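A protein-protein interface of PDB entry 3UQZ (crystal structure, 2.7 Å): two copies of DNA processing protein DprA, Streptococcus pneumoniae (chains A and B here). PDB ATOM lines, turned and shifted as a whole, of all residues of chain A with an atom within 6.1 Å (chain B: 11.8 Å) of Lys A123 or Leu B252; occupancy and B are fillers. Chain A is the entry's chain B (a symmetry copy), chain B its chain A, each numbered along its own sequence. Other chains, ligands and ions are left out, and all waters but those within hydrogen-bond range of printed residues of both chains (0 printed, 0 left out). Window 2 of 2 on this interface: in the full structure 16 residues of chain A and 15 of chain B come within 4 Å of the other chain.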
ATOM      1  N   SER A 118      -7.995  -7.019   9.232  1.00  0.00           N
ATOM      2  CA  SER A 118      -7.713  -7.810   8.036  1.00  0.00           C
ATOM      3  C   SER A 118      -6.646  -8.851   8.360  1.00  0.00           C
ATOM      4  O   SER A 118      -5.931  -8.696   9.353  1.00  0.00           O
ATOM      5  CB  SER A 118      -7.249  -6.912   6.891  1.00  0.00           C
ATOM      6  OG  SER A 118      -5.889  -6.536   7.046  1.00  0.00           O
ATOM      7  N   LYS A 119      -6.523  -9.897   7.517  1.00  0.00           N
ATOM      8  CA  LYS A 119      -5.530 -10.965   7.678  1.00  0.00           C
ATOM      9  C   LYS A 119      -4.107 -10.370   7.561  1.00  0.00           C
ATOM     10  O   LYS A 119      -3.147 -10.888   8.145  1.00  0.00           O
ATOM     11  CB  LYS A 119      -5.774 -12.054   6.612  1.00  0.00           C
ATOM     12  CG  LYS A 119      -5.007 -13.362   6.812  1.00  0.00           C
ATOM     13  CD  LYS A 119      -5.465 -14.447   5.826  1.00  0.00           C
ATOM     14  CE  LYS A 119      -4.355 -15.416   5.478  1.00  0.00           C
ATOM     15  NZ  LYS A 119      -4.757 -16.832   5.687  1.00  0.00           N
ATOM     16  N   GLN A 120      -4.004  -9.253   6.815  1.00  0.00           N
ATOM     17  CA  GLN A 120      -2.777  -8.495   6.572  1.00  0.00           C
ATOM     18  C   GLN A 120      -2.352  -7.875   7.905  1.00  0.00           C
ATOM     19  O   GLN A 120      -1.238  -8.117   8.381  1.00  0.00           O
ATOM     20  CB  GLN A 120      -3.031  -7.379   5.523  1.00  0.00           C
ATOM     21  CG  GLN A 120      -3.824  -7.795   4.270  1.00  0.00           C
ATOM     22  CD  GLN A 120      -5.039  -6.925   4.010  1.00  0.00           C
ATOM     23  OE1 GLN A 120      -4.994  -5.687   4.083  1.00  0.00           O
ATOM     24  NE2 GLN A 120      -6.156  -7.559   3.674  1.00  0.00           N
ATOM     25  N   GLY A 121      -3.293  -7.137   8.505  1.00  0.00           N
ATOM     26  CA  GLY A 121      -3.156  -6.452   9.783  1.00  0.00           C
ATOM     27  C   GLY A 121      -2.652  -7.351  10.889  1.00  0.00           C
ATOM     28  O   GLY A 121      -1.684  -6.996  11.571  1.00  0.00           O
ATOM     29  N   ALA A 122      -3.270  -8.552  11.031  1.00  0.00           N
ATOM     30  CA  ALA A 122      -2.878  -9.549  12.030  1.00  0.00           C
ATOM     31  C   ALA A 122      -1.463 -10.081  11.818  1.00  0.00           C
ATOM     32  O   ALA A 122      -0.734 -10.286  12.797  1.00  0.00           O
ATOM     33  CB  ALA A 122      -3.873 -10.688  12.059  1.00  0.00           C
ATOM     34  N   LYS A 123      -1.055 -10.277  10.558  1.00  0.00           N
ATOM     35  CA  LYS A 123       0.300 -10.742  10.266  1.00  0.00           C
ATOM     36  C   LYS A 123       1.336  -9.675  10.615  1.00  0.00           C
ATOM     37  O   LYS A 123       2.423  -9.986  11.113  1.00  0.00           O
ATOM     38  CB  LYS A 123       0.422 -11.131   8.794  1.00  0.00           C
ATOM     39  CG  LYS A 123       1.209 -12.411   8.557  1.00  0.00           C
ATOM     40  CD  LYS A 123       0.283 -13.605   8.382  1.00  0.00           C
ATOM     41  CE  LYS A 123       0.949 -14.709   7.587  1.00  0.00           C
ATOM     42  NZ  LYS A 123       0.977 -15.996   8.335  1.00  0.00           N
ATOM     43  N   SER A 124       0.991  -8.412  10.352  1.00  0.00           N
ATOM     44  CA  SER A 124       1.863  -7.270  10.625  1.00  0.00           C
ATOM     45  C   SER A 124       2.206  -7.218  12.116  1.00  0.00           C
ATOM     46  O   SER A 124       3.381  -7.079  12.467  1.00  0.00           O
ATOM     47  CB  SER A 124       1.186  -5.971  10.203  1.00  0.00           C
ATOM     48  OG  SER A 124       0.737  -6.015   8.859  1.00  0.00           O
ATOM     49  N   VAL A 125       1.179  -7.372  12.983  1.00  0.00           N
ATOM     50  CA  VAL A 125       1.308  -7.381  14.446  1.00  0.00           C
ATOM     51  C   VAL A 125       2.189  -8.553  14.881  1.00  0.00           C
ATOM     52  O   VAL A 125       3.131  -8.360  15.662  1.00  0.00           O
ATOM     53  CB  VAL A 125      -0.089  -7.390  15.116  1.00  0.00           C
ATOM     54  CG1 VAL A 125       0.000  -7.627  16.620  1.00  0.00           C
ATOM     55  CG2 VAL A 125      -0.830  -6.094  14.830  1.00  0.00           C
ATOM     56  N   GLU A 126       1.921  -9.751  14.346  1.00  0.00           N
ATOM     57  CA  GLU A 126       2.739 -10.921  14.658  1.00  0.00           C
ATOM     58  C   GLU A 126       4.207 -10.691  14.306  1.00  0.00           C
ATOM     59  O   GLU A 126       5.095 -10.942  15.127  1.00  0.00           O
ATOM     60  CB  GLU A 126       2.207 -12.146  13.920  1.00  0.00           C
ATOM     61  CG  GLU A 126       2.205 -13.417  14.749  1.00  0.00           C
ATOM     62  CD  GLU A 126       3.023 -14.533  14.128  1.00  0.00           C
ATOM     63  OE1 GLU A 126       3.152 -14.552  12.883  1.00  0.00           O
ATOM     64  OE2 GLU A 126       3.539 -15.388  14.883  1.00  0.00           O
ATOM     65  N   LYS A 127       4.462 -10.208  13.087  1.00  0.00           N
ATOM     66  CA  LYS A 127       5.821  -9.955  12.610  1.00  0.00           C
ATOM     67  C   LYS A 127       6.571  -9.017  13.556  1.00  0.00           C
ATOM     68  O   LYS A 127       7.688  -9.338  13.964  1.00  0.00           O
ATOM     69  CB  LYS A 127       5.789  -9.403  11.177  1.00  0.00           C
ATOM     70  CG  LYS A 127       7.154  -9.272  10.506  1.00  0.00           C
ATOM     71  CD  LYS A 127       7.009  -8.637   9.113  1.00  0.00           C
ATOM     72  CE  LYS A 127       8.326  -8.359   8.430  1.00  0.00           C
ATOM     73  NZ  LYS A 127       9.007  -7.159   8.986  1.00  0.00           N
ATOM     74  N   VAL A 128       5.938  -7.879  13.929  1.00  0.00           N
ATOM     75  CA  VAL A 128       6.506  -6.889  14.860  1.00  0.00           C
ATOM     76  C   VAL A 128       6.773  -7.534  16.234  1.00  0.00           C
ATOM     77  O   VAL A 128       7.866  -7.370  16.770  1.00  0.00           O
ATOM     78  CB  VAL A 128       5.654  -5.576  14.944  1.00  0.00           C
ATOM     79  CG1 VAL A 128       6.211  -4.601  15.978  1.00  0.00           C
ATOM     80  CG2 VAL A 128       5.558  -4.891  13.583  1.00  0.00           C
ATOM     81  N   ALA A 149      -4.739 -11.126  18.188  1.00  0.00           N
ATOM     82  CA  ALA A 149      -3.516 -11.434  17.435  1.00  0.00           C
ATOM     83  C   ALA A 149      -2.254 -11.097  18.214  1.00  0.00           C
ATOM     84  O   ALA A 149      -1.261 -11.822  18.101  1.00  0.00           O
ATOM     85  CB  ALA A 149      -3.516 -10.718  16.093  1.00  0.00           C
ATOM     86  N   SER B 118       3.599  -3.315  -7.965  1.00  0.00           N
ATOM     87  CA  SER B 118       2.340  -4.039  -7.816  1.00  0.00           C
ATOM     88  C   SER B 118       1.194  -3.181  -8.365  1.00  0.00           C
ATOM     89  O   SER B 118       1.357  -1.967  -8.540  1.00  0.00           O
ATOM     90  CB  SER B 118       2.097  -4.353  -6.341  1.00  0.00           C
ATOM     91  OG  SER B 118       1.692  -3.203  -5.618  1.00  0.00           O
ATOM     92  N   GLN B 120      -1.422  -2.333  -6.761  1.00  0.00           N
ATOM     93  CA  GLN B 120      -1.755  -1.448  -5.638  1.00  0.00           C
ATOM     94  C   GLN B 120      -0.845  -0.230  -5.632  1.00  0.00           C
ATOM     95  O   GLN B 120      -1.326   0.882  -5.422  1.00  0.00           O
ATOM     96  CB  GLN B 120      -1.692  -2.193  -4.289  1.00  0.00           C
ATOM     97  CG  GLN B 120      -2.751  -3.297  -4.120  1.00  0.00           C
ATOM     98  CD  GLN B 120      -4.165  -2.767  -4.005  1.00  0.00           C
ATOM     99  OE1 GLN B 120      -4.907  -2.686  -4.993  1.00  0.00           O
ATOM    100  NE2 GLN B 120      -4.576  -2.416  -2.790  1.00  0.00           N
ATOM    101  N   GLU B 223       6.536   2.538  -3.643  1.00  0.00           N
ATOM    102  CA  GLU B 223       7.089   1.200  -3.795  1.00  0.00           C
ATOM    103  C   GLU B 223       8.587   1.195  -4.071  1.00  0.00           C
ATOM    104  O   GLU B 223       9.036   0.611  -5.048  1.00  0.00           O
ATOM    105  CB  GLU B 223       6.274   0.340  -4.791  1.00  0.00           C
ATOM    106  CG  GLU B 223       4.836   0.108  -4.349  1.00  0.00           C
ATOM    107  CD  GLU B 223       4.176  -1.175  -4.809  1.00  0.00           C
ATOM    108  OE1 GLU B 223       4.658  -1.786  -5.792  1.00  0.00           O
ATOM    109  OE2 GLU B 223       3.142  -1.548  -4.208  1.00  0.00           O
ATOM    110  N   ALA B 224       9.355   1.844  -3.201  1.00  0.00           N
ATOM    111  CA  ALA B 224      10.807   1.851  -3.291  1.00  0.00           C
ATOM    112  C   ALA B 224      11.302   0.738  -2.372  1.00  0.00           C
ATOM    113  O   ALA B 224      10.895   0.664  -1.212  1.00  0.00           O
ATOM    114  CB  ALA B 224      11.363   3.201  -2.861  1.00  0.00           C
ATOM    115  N   LYS B 225      12.062  -0.203  -2.936  1.00  0.00           N
ATOM    116  CA  LYS B 225      12.631  -1.328  -2.198  1.00  0.00           C
ATOM    117  C   LYS B 225      13.904  -0.852  -1.520  1.00  0.00           C
ATOM    118  O   LYS B 225      14.385   0.243  -1.816  1.00  0.00           O
ATOM    119  CB  LYS B 225      12.966  -2.487  -3.145  1.00  0.00           C
ATOM    120  CG  LYS B 225      11.754  -3.251  -3.617  1.00  0.00           C
ATOM    121  CD  LYS B 225      12.100  -4.105  -4.791  1.00  0.00           C
ATOM    122  CE  LYS B 225      10.868  -4.376  -5.604  1.00  0.00           C
ATOM    123  NZ  LYS B 225      11.092  -5.475  -6.577  1.00  0.00           N
ATOM    124  N   MET B 226      14.452  -1.653  -0.603  1.00  0.00           N
ATOM    125  CA  MET B 226      15.721  -1.306   0.019  1.00  0.00           C
ATOM    126  C   MET B 226      16.788  -1.476  -1.056  1.00  0.00           C
ATOM    127  O   MET B 226      16.626  -2.304  -1.955  1.00  0.00           O
ATOM    128  CB  MET B 226      16.015  -2.215   1.212  1.00  0.00           C
ATOM    129  CG  MET B 226      15.191  -1.878   2.433  1.00  0.00           C
ATOM    130  SD  MET B 226      15.458  -0.075   3.144  1.00  0.00           S
ATOM    131  CE  MET B 226      14.577  -0.378   4.859  1.00  0.00           C
ATOM    132  N   PRO B 248       3.121   5.283   1.876  1.00  0.00           N
ATOM    133  CA  PRO B 248       3.342   4.032   2.625  1.00  0.00           C
ATOM    134  C   PRO B 248       2.630   2.831   2.009  1.00  0.00           C
ATOM    135  O   PRO B 248       1.795   2.977   1.116  1.00  0.00           O
ATOM    136  CB  PRO B 248       2.800   4.353   4.023  1.00  0.00           C
ATOM    137  CG  PRO B 248       1.741   5.378   3.787  1.00  0.00           C
ATOM    138  CD  PRO B 248       2.126   6.149   2.550  1.00  0.00           C
ATOM    139  N   GLY B 249       2.989   1.654   2.497  1.00  0.00           N
ATOM    140  CA  GLY B 249       2.403   0.392   2.071  1.00  0.00           C
ATOM    141  C   GLY B 249       2.491  -0.667   3.148  1.00  0.00           C
ATOM    142  O   GLY B 249       2.797  -0.357   4.304  1.00  0.00           O
ATOM    143  N   SER B 250       2.244  -1.931   2.759  1.00  0.00           N
ATOM    144  CA  SER B 250       2.317  -3.103   3.624  1.00  0.00           C
ATOM    145  C   SER B 250       3.743  -3.286   4.113  1.00  0.00           C
ATOM    146  O   SER B 250       4.675  -2.994   3.370  1.00  0.00           O
ATOM    147  CB  SER B 250       1.879  -4.347   2.852  1.00  0.00           C
ATOM    148  OG  SER B 250       2.250  -5.556   3.500  1.00  0.00           O
ATOM    149  N   ILE B 251       3.919  -3.782   5.343  1.00  0.00           N
ATOM    150  CA  ILE B 251       5.259  -4.047   5.893  1.00  0.00           C
ATOM    151  C   ILE B 251       5.693  -5.486   5.580  1.00  0.00           C
ATOM    152  O   ILE B 251       6.826  -5.882   5.889  1.00  0.00           O
ATOM    153  CB  ILE B 251       5.368  -3.701   7.404  1.00  0.00           C
ATOM    154  CG1 ILE B 251       4.388  -4.523   8.273  1.00  0.00           C
ATOM    155  CG2 ILE B 251       5.234  -2.201   7.631  1.00  0.00           C
ATOM    156  CD1 ILE B 251       5.048  -5.168   9.451  1.00  0.00           C
ATOM    157  N   LEU B 252       4.774  -6.251   4.946  1.00  0.00           N
ATOM    158  CA  LEU B 252       4.941  -7.660   4.591  1.00  0.00           C
ATOM    159  C   LEU B 252       5.668  -7.891   3.268  1.00  0.00           C
ATOM    160  O   LEU B 252       6.602  -8.688   3.259  1.00  0.00           O
ATOM    161  CB  LEU B 252       3.588  -8.399   4.593  1.00  0.00           C
ATOM    162  CG  LEU B 252       2.698  -8.249   5.856  1.00  0.00           C
ATOM    163  CD1 LEU B 252       1.216  -8.343   5.507  1.00  0.00           C
ATOM    164  CD2 LEU B 252       3.065  -9.261   6.922  1.00  0.00           C
ATOM    165  N   ASP B 253       5.252  -7.192   2.166  1.00  0.00           N
ATOM    166  CA  ASP B 253       5.780  -7.294   0.780  1.00  0.00           C
ATOM    167  C   ASP B 253       7.259  -7.080   0.565  1.00  0.00           C
ATOM    168  O   ASP B 253       7.816  -7.679  -0.357  1.00  0.00           O
ATOM    169  CB  ASP B 253       5.131  -6.258  -0.157  1.00  0.00           C
ATOM    170  CG  ASP B 253       3.644  -6.311  -0.337  1.00  0.00           C
ATOM    171  OD1 ASP B 253       3.106  -7.426  -0.483  1.00  0.00           O
ATOM    172  OD2 ASP B 253       3.039  -5.235  -0.519  1.00  0.00           O
ATOM    173  N   GLY B 254       7.838  -6.099   1.249  1.00  0.00           N
ATOM    174  CA  GLY B 254       9.224  -5.705   1.014  1.00  0.00           C
ATOM    175  C   GLY B 254       9.308  -4.595  -0.025  1.00  0.00           C
ATOM    176  O   GLY B 254      10.340  -3.926  -0.159  1.00  0.00           O
ATOM    177  N   LEU B 255       8.193  -4.383  -0.752  1.00  0.00           N
ATOM    178  CA  LEU B 255       8.022  -3.381  -1.793  1.00  0.00           C
ATOM    179  C   LEU B 255       8.125  -1.940  -1.312  1.00  0.00           C
ATOM    180  O   LEU B 255       8.680  -1.124  -2.038  1.00  0.00           O
ATOM    181  CB  LEU B 255       6.677  -3.584  -2.504  1.00  0.00           C
ATOM    182  CG  LEU B 255       6.657  -4.592  -3.643  1.00  0.00           C
ATOM    183  CD1 LEU B 255       5.251  -5.030  -3.923  1.00  0.00           C
ATOM    184  CD2 LEU B 255       7.288  -4.014  -4.908  1.00  0.00           C
ATOM    185  N   SER B 256       7.575  -1.607  -0.125  1.00  0.00           N
ATOM    186  CA  SER B 256       7.597  -0.230   0.383  1.00  0.00           C
ATOM    187  C   SER B 256       8.622   0.033   1.493  1.00  0.00           C
ATOM    188  O   SER B 256       8.530   1.056   2.172  1.00  0.00           O
ATOM    189  CB  SER B 256       6.199   0.206   0.809  1.00  0.00           C
ATOM    190  OG  SER B 256       5.324   0.295  -0.303  1.00  0.00           O
ATOM    191  N   ASP B 257       9.617  -0.862   1.644  1.00  0.00           N
ATOM    192  CA  ASP B 257      10.653  -0.777   2.675  1.00  0.00           C
ATOM    193  C   ASP B 257      11.477   0.495   2.602  1.00  0.00           C
ATOM    194  O   ASP B 257      11.826   1.054   3.639  1.00  0.00           O
ATOM    195  CB  ASP B 257      11.570  -2.020   2.655  1.00  0.00           C
ATOM    196  CG  ASP B 257      10.969  -3.345   3.126  1.00  0.00           C
ATOM    197  OD1 ASP B 257       9.747  -3.383   3.422  1.00  0.00           O
ATOM    198  OD2 ASP B 257      11.717  -4.354   3.170  1.00  0.00           O
ATOM    199  N   GLY B 258      11.785   0.931   1.386  1.00  0.00           N
ATOM    200  CA  GLY B 258      12.565   2.136   1.125  1.00  0.00           C
ATOM    201  C   GLY B 258      11.810   3.397   1.482  1.00  0.00           C
ATOM    202  O   GLY B 258      12.395   4.325   2.038  1.00  0.00           O
ATOM    203  N   CYS B 259      10.489   3.423   1.179  1.00  0.00           N
ATOM    204  CA  CYS B 259       9.559   4.509   1.505  1.00  0.00           C
ATOM    205  C   CYS B 259       9.495   4.664   3.011  1.00  0.00           C
ATOM    206  O   CYS B 259       9.552   5.782   3.516  1.00  0.00           O
ATOM    207  CB  CYS B 259       8.167   4.227   0.944  1.00  0.00           C
ATOM    208  SG  CYS B 259       8.089   4.090  -0.858  1.00  0.00           S
ATOM    209  N   HIS B 260       9.361   3.528   3.722  1.00  0.00           N
ATOM    210  CA  HIS B 260       9.266   3.453   5.175  1.00  0.00           C
ATOM    211  C   HIS B 260      10.543   3.935   5.831  1.00  0.00           C
ATOM    212  O   HIS B 260      10.469   4.701   6.792  1.00  0.00           O
ATOM    213  CB  HIS B 260       8.880   2.035   5.621  1.00  0.00           C
ATOM    214  CG  HIS B 260       7.513   1.609   5.175  1.00  0.00           C
ATOM    215  ND1 HIS B 260       7.158   0.277   5.148  1.00  0.00           N
ATOM    216  CD2 HIS B 260       6.462   2.351   4.746  1.00  0.00           C
ATOM    217  CE1 HIS B 260       5.909   0.247   4.711  1.00  0.00           C
ATOM    218  NE2 HIS B 260       5.450   1.471   4.450  1.00  0.00           N
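The side-chain hydroxyl (OG) of Ser B250 is in hydrogen-bond range of the backbone NH (N) of Leu B252 (3.0 Å). The side-chain hydroxyl (OG) of Ser A118 sits close to the side-chain amide oxygen (OE1) of Gln A120 (3.2 Å). The backbone carbonyl oxygen of Gln A120 sits at hydrogen-bond distance from the side-chain hydroxyl of Ser A124, at 2.9 Å.
Among the printed residues, merely in contact across the chains: Gln A120 with Leu B252 (3.8 Å), Lys A123 with Leu B252 (3.7 Å), Ser A124 with Ile B251 (3.9 Å) and Lys A127 with Ile B251 (3.9 Å).
Of chain B, only Leu B252 (3.7 Å) comes within 4 Å of Lys A123. Leu B252 touches two residues of chain A. Lys A119 touches none of the printed residues of chain B. No residue of chain B comes within 4 Å of Gly A121. No residue of chain B comes within 4 Å of Ala A122. No residue of chain B comes within 4 Å of Val A125. No residue of chain B comes within 4 Å of Glu A126. Lys A127 touches just one residue of chain B: Ile B251 (3.9 Å). Of the printed residues of chain A, Ile B251 touches Ser A124 (3.9 Å) and Lys A127 (3.9 Å). Met B226 touches none of the printed residues of chain A. The nearest residue of chain B that does not touch Lys A123 is Ile B251 (5.7 Å). The nearest printed residue of chain A that does not touch Ile B251 is Val A128 (4.2 Å).
Hydrophobic or aromatic side chains of chain B within 4 Å of the printed part of chain A: Ile B251 and Leu B252. Among the printed residues, 4 pairs touch across the chains.
Positions printed for both chains: 118 and 120.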
